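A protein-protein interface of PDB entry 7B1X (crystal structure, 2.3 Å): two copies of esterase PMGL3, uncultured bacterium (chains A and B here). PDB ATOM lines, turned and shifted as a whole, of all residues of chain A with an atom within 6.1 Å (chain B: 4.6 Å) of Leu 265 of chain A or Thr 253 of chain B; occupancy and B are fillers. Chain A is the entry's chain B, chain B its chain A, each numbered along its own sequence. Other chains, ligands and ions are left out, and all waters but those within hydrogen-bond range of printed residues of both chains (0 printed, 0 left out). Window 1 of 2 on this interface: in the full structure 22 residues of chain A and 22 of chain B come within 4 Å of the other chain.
The backbone NH (N) of Leu 265 of chain B lies within hydrogen-bond range of the backbone carbonyl oxygen (O) of Leu 265 of chain A, at 2.7 Å.
O of Val 263 of chain B lies within hydrogen-bond range of N of Val 267 of chain A.
A ring nitrogen (ND1) of His 266 of chain A sits close to the guanidinium group (NH2) of Arg 264 of chain B (3.5 Å).
O of Ser 249 of chain B sits at hydrogen-bond distance from OG1 of Thr 253 of chain B, at 2.8 Å.
The side-chain carboxylate of Glu 251 of chain B is in salt-bridge range of the guanidinium group of Arg 254 of chain B, at 2.7 Å.
N of Val 239 of chain A sits at hydrogen-bond distance from O of His 266 of chain A, at 3.0 Å.
N of Ile 237 of chain A is in hydrogen-bond range of O of Arg 264 of chain A, 2.8 Å away.
O of Arg 264 of chain B lies within hydrogen-bond range of N of Ile 237 of chain B (2.8 Å).
N of Arg 264 of chain A is in hydrogen-bond range of O of Leu 235 of chain A, at 2.9 Å.
CB of Arg 254 of chain B touches CG1 of Val 250 of chain A, at 3.7 Å.
Leu 265 of chain B touches Val 263 of chain A (O to O, 3.7 Å).
Arg 264 of chain A touches Leu 265 of chain B.
Leu 265 of chain A touches Thr 253 of chain B.
Leu 265 of chain A touches Val 263 of chain B (O to O, 3.8 Å).
O of Leu 265 of chain A touches CA of Arg 264 of chain B (3.3 Å).
His 266 of chain A touches Val 263 of chain B.
CG2 of Val 267 of chain A touches CB of Ala 257 of chain B, 3.9 Å away.
Of chain B, only Thr 253, Val 263, Arg 264 and Leu 265 come within 4 Å of Leu 265 of chain A.
Of the printed residues of chain A, Thr 253 of chain B touches Leu 265.
Of the printed residues of chain B, His 266 of chain A touches Val 263 (3.6 Å) and Arg 264 (3.1 Å).
Printed residues of chain B within 4 Å of Val 250 of chain A: Arg 254 (3.7 Å).
Printed residues of chain B within 4 Å of Val 267 of chain A: Ala 257 and Val 263.
Glu 251 of chain B touches none of the printed residues of chain A.
The nearest printed residue of chain B that does not touch Leu 265 of chain A is Ala 257 of chain B (6.2 Å).
Of the 13 printed residues of chain B, 6 touch a printed residue of chain A.
Of the 13 printed residues of chain A, 6 touch a printed residue of chain B.
Among the printed residues, 11 pairs touch across the chains.
Among the printed residues, no Asp or Glu carboxylate lies within 4 Å of a Lys or Arg side-chain nitrogen of the other chain.
Val 263 of chain A touches Leu 265 of chain B, and with the chains exchanged Leu 265 of chain A touches Val 263 of chain B.
Arg 264 of chain A touches Leu 265 of chain B, and with the chains exchanged Leu 265 of chain A touches Arg 264 of chain B.
Leu 265 of chain A touches Thr 253 of chain B, but with the chains exchanged Thr 253 of chain A does not touch Leu 265 of chain B (4.2 Å).
Leu 265 of chain B touches its own counterpart, Leu 265 of chain A.
Positions printed for both chains: 237, 249, 250, 253, 263, 264 and 265.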
ATOM      1  N   LEU A 235      -6.158  -8.378 -10.541  1.00  0.00           N
ATOM      2  CA  LEU A 235      -6.707  -7.843  -9.309  1.00  0.00           C
ATOM      3  C   LEU A 235      -6.039  -6.508  -8.983  1.00  0.00           C
ATOM      4  O   LEU A 235      -4.803  -6.362  -9.043  1.00  0.00           O
ATOM      5  CB  LEU A 235      -6.372  -8.812  -8.196  1.00  0.00           C
ATOM      6  CG  LEU A 235      -7.390  -9.803  -7.648  1.00  0.00           C
ATOM      7  CD1 LEU A 235      -8.333 -10.412  -8.651  1.00  0.00           C
ATOM      8  CD2 LEU A 235      -6.658 -10.919  -6.914  1.00  0.00           C
ATOM      9  N   PHE A 236      -6.877  -5.555  -8.566  1.00  0.00           N
ATOM     10  CA  PHE A 236      -6.371  -4.409  -7.859  1.00  0.00           C
ATOM     11  C   PHE A 236      -7.059  -4.322  -6.515  1.00  0.00           C
ATOM     12  O   PHE A 236      -8.281  -4.314  -6.470  1.00  0.00           O
ATOM     13  CB  PHE A 236      -6.580  -3.141  -8.692  1.00  0.00           C
ATOM     14  CG  PHE A 236      -6.174  -1.867  -8.010  1.00  0.00           C
ATOM     15  CD1 PHE A 236      -4.944  -1.776  -7.359  1.00  0.00           C
ATOM     16  CD2 PHE A 236      -7.022  -0.768  -7.997  1.00  0.00           C
ATOM     17  CE1 PHE A 236      -4.543  -0.598  -6.729  1.00  0.00           C
ATOM     18  CE2 PHE A 236      -6.614   0.422  -7.386  1.00  0.00           C
ATOM     19  CZ  PHE A 236      -5.378   0.511  -6.762  1.00  0.00           C
ATOM     20  N   ILE A 237      -6.253  -4.270  -5.446  1.00  0.00           N
ATOM     21  CA  ILE A 237      -6.752  -4.195  -4.082  1.00  0.00           C
ATOM     22  C   ILE A 237      -6.171  -2.976  -3.387  1.00  0.00           C
ATOM     23  O   ILE A 237      -4.944  -2.760  -3.340  1.00  0.00           O
ATOM     24  CB  ILE A 237      -6.414  -5.471  -3.287  1.00  0.00           C
ATOM     25  CG1 ILE A 237      -6.864  -6.745  -4.012  1.00  0.00           C
ATOM     26  CG2 ILE A 237      -6.988  -5.379  -1.871  1.00  0.00           C
ATOM     27  CD1 ILE A 237      -6.286  -8.041  -3.387  1.00  0.00           C
ATOM     28  N   GLN A 238      -7.085  -2.184  -2.820  1.00  0.00           N
ATOM     29  CA  GLN A 238      -6.712  -1.057  -1.981  1.00  0.00           C
ATOM     30  C   GLN A 238      -7.174  -1.411  -0.604  1.00  0.00           C
ATOM     31  O   GLN A 238      -8.319  -1.879  -0.434  1.00  0.00           O
ATOM     32  CB  GLN A 238      -7.607   0.151  -2.307  1.00  0.00           C
ATOM     33  CG  GLN A 238      -6.950   1.130  -3.284  1.00  0.00           C
ATOM     34  CD  GLN A 238      -7.812   2.232  -3.848  1.00  0.00           C
ATOM     35  OE1 GLN A 238      -9.063   2.249  -3.736  1.00  0.00           O
ATOM     36  NE2 GLN A 238      -7.143   3.150  -4.537  1.00  0.00           N
ATOM     37  N   VAL A 239      -6.306  -1.186   0.389  1.00  0.00           N
ATOM     38  CA  VAL A 239      -6.778  -1.418   1.744  1.00  0.00           C
ATOM     39  C   VAL A 239      -6.011  -0.406   2.620  1.00  0.00           C
ATOM     40  O   VAL A 239      -4.939   0.089   2.218  1.00  0.00           O
ATOM     41  CB  VAL A 239      -6.524  -2.925   2.079  1.00  0.00           C
ATOM     42  CG1 VAL A 239      -5.028  -3.271   1.988  1.00  0.00           C
ATOM     43  CG2 VAL A 239      -7.113  -3.328   3.417  1.00  0.00           C
ATOM     44  N   SER A 249      -6.823  -8.760   2.842  1.00  0.00           N
ATOM     45  CA  SER A 249      -6.252  -8.239   1.616  1.00  0.00           C
ATOM     46  C   SER A 249      -4.887  -8.844   1.303  1.00  0.00           C
ATOM     47  O   SER A 249      -4.672  -9.270   0.168  1.00  0.00           O
ATOM     48  CB  SER A 249      -6.185  -6.757   1.684  1.00  0.00           C
ATOM     49  OG  SER A 249      -7.490  -6.279   1.431  1.00  0.00           O
ATOM     50  N   VAL A 250      -3.983  -8.855   2.277  1.00  0.00           N
ATOM     51  CA  VAL A 250      -2.673  -9.437   2.057  1.00  0.00           C
ATOM     52  C   VAL A 250      -2.751 -10.927   1.703  1.00  0.00           C
ATOM     53  O   VAL A 250      -2.057 -11.380   0.802  1.00  0.00           O
ATOM     54  CB  VAL A 250      -1.672  -9.163   3.189  1.00  0.00           C
ATOM     55  CG1 VAL A 250      -0.308  -9.657   2.746  1.00  0.00           C
ATOM     56  CG2 VAL A 250      -1.626  -7.659   3.554  1.00  0.00           C
ATOM     57  N   THR A 253      -4.040 -11.436  -1.792  1.00  0.00           N
ATOM     58  CA  THR A 253      -2.891 -11.083  -2.616  1.00  0.00           C
ATOM     59  C   THR A 253      -1.934 -12.269  -2.717  1.00  0.00           C
ATOM     60  O   THR A 253      -1.585 -12.719  -3.800  1.00  0.00           O
ATOM     61  CB  THR A 253      -2.209  -9.814  -2.090  1.00  0.00           C
ATOM     62  OG1 THR A 253      -3.225  -8.814  -2.142  1.00  0.00           O
ATOM     63  CG2 THR A 253      -1.119  -9.386  -3.041  1.00  0.00           C
ATOM     64  N   VAL A 263      -1.451  -9.053  -9.776  1.00  0.00           N
ATOM     65  CA  VAL A 263      -2.110  -8.505  -8.607  1.00  0.00           C
ATOM     66  C   VAL A 263      -1.370  -7.291  -8.109  1.00  0.00           C
ATOM     67  O   VAL A 263      -0.184  -7.284  -7.952  1.00  0.00           O
ATOM     68  CB  VAL A 263      -2.460  -9.530  -7.482  1.00  0.00           C
ATOM     69  CG1 VAL A 263      -1.287 -10.428  -7.072  1.00  0.00           C
ATOM     70  CG2 VAL A 263      -3.037  -8.796  -6.253  1.00  0.00           C
ATOM     71  N   ARG A 264      -2.122  -6.219  -7.969  1.00  0.00           N
ATOM     72  CA  ARG A 264      -1.637  -4.960  -7.450  1.00  0.00           C
ATOM     73  C   ARG A 264      -2.343  -4.752  -6.113  1.00  0.00           C
ATOM     74  O   ARG A 264      -3.570  -4.801  -6.050  1.00  0.00           O
ATOM     75  CB  ARG A 264      -2.084  -3.814  -8.383  1.00  0.00           C
ATOM     76  CG  ARG A 264      -1.123  -3.367  -9.477  1.00  0.00           C
ATOM     77  CD  ARG A 264      -1.227  -1.995 -10.174  1.00  0.00           C
ATOM     78  NE  ARG A 264      -1.538  -2.159 -11.600  1.00  0.00           N
ATOM     79  CZ  ARG A 264      -0.787  -1.784 -12.652  1.00  0.00           C
ATOM     80  NH1 ARG A 264       0.384  -1.187 -12.471  1.00  0.00           N
ATOM     81  NH2 ARG A 264      -1.205  -2.047 -13.893  1.00  0.00           N
ATOM     82  N   LEU A 265      -1.556  -4.533  -5.063  1.00  0.00           N
ATOM     83  CA  LEU A 265      -2.020  -4.263  -3.708  1.00  0.00           C
ATOM     84  C   LEU A 265      -1.384  -2.956  -3.262  1.00  0.00           C
ATOM     85  O   LEU A 265      -0.131  -2.825  -3.315  1.00  0.00           O
ATOM     86  CB  LEU A 265      -1.576  -5.384  -2.747  1.00  0.00           C
ATOM     87  CG  LEU A 265      -1.845  -5.107  -1.263  1.00  0.00           C
ATOM     88  CD1 LEU A 265      -3.338  -4.993  -0.956  1.00  0.00           C
ATOM     89  CD2 LEU A 265      -1.141  -6.120  -0.355  1.00  0.00           C
ATOM     90  N   HIS A 266      -2.256  -2.003  -2.900  1.00  0.00           N
ATOM     91  CA  HIS A 266      -1.813  -0.747  -2.317  1.00  0.00           C
ATOM     92  C   HIS A 266      -2.324  -0.686  -0.886  1.00  0.00           C
ATOM     93  O   HIS A 266      -3.544  -0.614  -0.704  1.00  0.00           O
ATOM     94  CB  HIS A 266      -2.060   0.520  -3.200  1.00  0.00           C
ATOM     95  CG  HIS A 266      -1.316   1.748  -2.637  1.00  0.00           C
ATOM     96  ND1 HIS A 266      -1.298   3.028  -3.268  1.00  0.00           N
ATOM     97  CD2 HIS A 266      -0.545   1.915  -1.513  1.00  0.00           C
ATOM     98  CE1 HIS A 266      -0.541   3.863  -2.548  1.00  0.00           C
ATOM     99  NE2 HIS A 266      -0.054   3.189  -1.466  1.00  0.00           N
ATOM    100  N   VAL A 267      -1.374  -0.795   0.070  1.00  0.00           N
ATOM    101  CA  VAL A 267      -1.670  -0.505   1.463  1.00  0.00           C
ATOM    102  C   VAL A 267      -1.381   0.961   1.756  1.00  0.00           C
ATOM    103  O   VAL A 267      -0.221   1.371   1.662  1.00  0.00           O
ATOM    104  CB  VAL A 267      -0.977  -1.419   2.491  1.00  0.00           C
ATOM    105  CG1 VAL A 267      -1.558  -1.093   3.845  1.00  0.00           C
ATOM    106  CG2 VAL A 267      -1.173  -2.919   2.200  1.00  0.00           C
ATOM    107  N   ILE B 237       7.272  -2.498  -4.050  1.00  0.00           N
ATOM    108  CA  ILE B 237       7.868  -3.754  -4.447  1.00  0.00           C
ATOM    109  C   ILE B 237       7.235  -4.243  -5.750  1.00  0.00           C
ATOM    110  O   ILE B 237       6.024  -4.470  -5.826  1.00  0.00           O
ATOM    111  CB  ILE B 237       7.702  -4.804  -3.329  1.00  0.00           C
ATOM    112  CG1 ILE B 237       8.270  -4.279  -2.010  1.00  0.00           C
ATOM    113  CG2 ILE B 237       8.262  -6.160  -3.755  1.00  0.00           C
ATOM    114  CD1 ILE B 237       7.618  -4.884  -0.788  1.00  0.00           C
ATOM    115  N   SER B 249       8.715 -11.348  -1.343  1.00  0.00           N
ATOM    116  CA  SER B 249       8.030 -10.095  -1.606  1.00  0.00           C
ATOM    117  C   SER B 249       6.684 -10.002  -0.879  1.00  0.00           C
ATOM    118  O   SER B 249       6.432  -8.991  -0.224  1.00  0.00           O
ATOM    119  CB  SER B 249       7.822  -9.902  -3.075  1.00  0.00           C
ATOM    120  OG  SER B 249       9.032  -9.547  -3.627  1.00  0.00           O
ATOM    121  N   VAL B 250       5.821 -11.023  -1.045  1.00  0.00           N
ATOM    122  CA  VAL B 250       4.549 -11.004  -0.336  1.00  0.00           C
ATOM    123  C   VAL B 250       4.732 -10.929   1.188  1.00  0.00           C
ATOM    124  O   VAL B 250       4.028 -10.161   1.836  1.00  0.00           O
ATOM    125  CB  VAL B 250       3.610 -12.146  -0.752  1.00  0.00           C
ATOM    126  CG1 VAL B 250       2.310 -12.121   0.054  1.00  0.00           C
ATOM    127  CG2 VAL B 250       3.358 -12.122  -2.259  1.00  0.00           C
ATOM    128  N   GLU B 251       5.689 -11.661   1.761  1.00  0.00           N
ATOM    129  CA  GLU B 251       5.910 -11.648   3.212  1.00  0.00           C
ATOM    130  C   GLU B 251       6.408 -10.282   3.692  1.00  0.00           C
ATOM    131  O   GLU B 251       5.955  -9.772   4.733  1.00  0.00           O
ATOM    132  CB  GLU B 251       6.841 -12.797   3.664  1.00  0.00           C
ATOM    133  CG  GLU B 251       7.144 -12.771   5.168  1.00  0.00           C
ATOM    134  CD  GLU B 251       5.989 -13.073   6.135  1.00  0.00           C
ATOM    135  OE1 GLU B 251       4.913 -13.545   5.683  1.00  0.00           O
ATOM    136  OE2 GLU B 251       6.157 -12.871   7.368  1.00  0.00           O
ATOM    137  N   PHE B 252       7.342  -9.695   2.939  1.00  0.00           N
ATOM    138  CA  PHE B 252       7.825  -8.404   3.358  1.00  0.00           C
ATOM    139  C   PHE B 252       6.640  -7.406   3.351  1.00  0.00           C
ATOM    140  O   PHE B 252       6.523  -6.531   4.213  1.00  0.00           O
ATOM    141  CB  PHE B 252       8.957  -8.009   2.408  1.00  0.00           C
ATOM    142  CG  PHE B 252       9.885  -6.987   2.995  1.00  0.00           C
ATOM    143  CD1 PHE B 252      10.760  -7.336   4.015  1.00  0.00           C
ATOM    144  CD2 PHE B 252       9.884  -5.671   2.539  1.00  0.00           C
ATOM    145  CE1 PHE B 252      11.584  -6.388   4.606  1.00  0.00           C
ATOM    146  CE2 PHE B 252      10.707  -4.717   3.140  1.00  0.00           C
ATOM    147  CZ  PHE B 252      11.554  -5.072   4.163  1.00  0.00           C
ATOM    148  N   THR B 253       5.785  -7.520   2.328  1.00  0.00           N
ATOM    149  CA  THR B 253       4.599  -6.694   2.173  1.00  0.00           C
ATOM    150  C   THR B 253       3.711  -6.875   3.408  1.00  0.00           C
ATOM    151  O   THR B 253       3.318  -5.908   4.045  1.00  0.00           O
ATOM    152  CB  THR B 253       3.905  -6.982   0.830  1.00  0.00           C
ATOM    153  OG1 THR B 253       4.863  -6.642  -0.187  1.00  0.00           O
ATOM    154  CG2 THR B 253       2.584  -6.244   0.715  1.00  0.00           C
ATOM    155  N   ARG B 254       3.421  -8.134   3.729  1.00  0.00           N
ATOM    156  CA  ARG B 254       2.588  -8.464   4.870  1.00  0.00           C
ATOM    157  C   ARG B 254       3.131  -7.738   6.092  1.00  0.00           C
ATOM    158  O   ARG B 254       2.369  -7.050   6.779  1.00  0.00           O
ATOM    159  CB  ARG B 254       2.554  -9.991   5.018  1.00  0.00           C
ATOM    160  CG  ARG B 254       1.441 -10.559   5.900  1.00  0.00           C
ATOM    161  CD  ARG B 254       1.771 -12.066   5.938  1.00  0.00           C
ATOM    162  NE  ARG B 254       1.532 -12.199   7.325  1.00  0.00           N
ATOM    163  CZ  ARG B 254       2.364 -12.336   8.339  1.00  0.00           C
ATOM    164  NH1 ARG B 254       3.649 -12.583   8.182  1.00  0.00           N
ATOM    165  NH2 ARG B 254       1.802 -12.314   9.540  1.00  0.00           N
ATOM    166  N   ARG B 255       4.455  -7.875   6.324  1.00  0.00           N
ATOM    167  CA  ARG B 255       5.057  -7.354   7.534  1.00  0.00           C
ATOM    168  C   ARG B 255       5.028  -5.840   7.527  1.00  0.00           C
ATOM    169  O   ARG B 255       4.831  -5.264   8.583  1.00  0.00           O
ATOM    170  CB  ARG B 255       6.447  -7.941   7.798  1.00  0.00           C
ATOM    171  CG  ARG B 255       6.351  -9.336   8.380  1.00  0.00           C
ATOM    172  CD  ARG B 255       7.430 -10.322   7.883  1.00  0.00           C
ATOM    173  NE  ARG B 255       8.330 -10.437   8.999  1.00  0.00           N
ATOM    174  CZ  ARG B 255       8.412 -11.383   9.882  1.00  0.00           C
ATOM    175  NH1 ARG B 255       9.186 -11.137  10.916  1.00  0.00           N
ATOM    176  NH2 ARG B 255       7.859 -12.558   9.710  1.00  0.00           N
ATOM    177  N   ALA B 256       5.305  -5.218   6.355  1.00  0.00           N
ATOM    178  CA  ALA B 256       5.296  -3.759   6.213  1.00  0.00           C
ATOM    179  C   ALA B 256       3.895  -3.232   6.546  1.00  0.00           C
ATOM    180  O   ALA B 256       3.738  -2.355   7.404  1.00  0.00           O
ATOM    181  CB  ALA B 256       5.792  -3.316   4.850  1.00  0.00           C
ATOM    182  N   ALA B 257       2.884  -3.891   5.991  1.00  0.00           N
ATOM    183  CA  ALA B 257       1.482  -3.531   6.186  1.00  0.00           C
ATOM    184  C   ALA B 257       1.129  -3.653   7.667  1.00  0.00           C
ATOM    185  O   ALA B 257       0.473  -2.776   8.263  1.00  0.00           O
ATOM    186  CB  ALA B 257       0.597  -4.412   5.327  1.00  0.00           C
ATOM    187  N   VAL B 263       2.612   0.616   1.707  1.00  0.00           N
ATOM    188  CA  VAL B 263       3.282  -0.406   0.921  1.00  0.00           C
ATOM    189  C   VAL B 263       2.480  -0.714  -0.319  1.00  0.00           C
ATOM    190  O   VAL B 263       1.281  -0.891  -0.303  1.00  0.00           O
ATOM    191  CB  VAL B 263       3.737  -1.675   1.706  1.00  0.00           C
ATOM    192  CG1 VAL B 263       2.650  -2.322   2.523  1.00  0.00           C
ATOM    193  CG2 VAL B 263       4.316  -2.702   0.734  1.00  0.00           C
ATOM    194  N   ARG B 264       3.168  -0.640  -1.426  1.00  0.00           N
ATOM    195  CA  ARG B 264       2.605  -1.006  -2.715  1.00  0.00           C
ATOM    196  C   ARG B 264       3.337  -2.250  -3.220  1.00  0.00           C
ATOM    197  O   ARG B 264       4.588  -2.276  -3.250  1.00  0.00           O
ATOM    198  CB  ARG B 264       2.886   0.142  -3.705  1.00  0.00           C
ATOM    199  CG  ARG B 264       1.847   1.246  -3.811  1.00  0.00           C
ATOM    200  CD  ARG B 264       2.112   1.697  -5.246  1.00  0.00           C
ATOM    201  NE  ARG B 264       1.327   2.865  -5.609  1.00  0.00           N
ATOM    202  CZ  ARG B 264       1.382   4.041  -4.987  1.00  0.00           C
ATOM    203  NH1 ARG B 264       2.198   4.242  -3.955  1.00  0.00           N
ATOM    204  NH2 ARG B 264       0.600   5.013  -5.403  1.00  0.00           N
ATOM    205  N   LEU B 265       2.560  -3.270  -3.637  1.00  0.00           N
ATOM    206  CA  LEU B 265       3.130  -4.490  -4.224  1.00  0.00           C
ATOM    207  C   LEU B 265       2.485  -4.731  -5.578  1.00  0.00           C
ATOM    208  O   LEU B 265       1.254  -4.697  -5.684  1.00  0.00           O
ATOM    209  CB  LEU B 265       2.915  -5.654  -3.263  1.00  0.00           C
ATOM    210  CG  LEU B 265       3.134  -7.092  -3.761  1.00  0.00           C
ATOM    211  CD1 LEU B 265       4.591  -7.329  -4.167  1.00  0.00           C
ATOM    212  CD2 LEU B 265       2.858  -8.050  -2.621  1.00  0.00           C
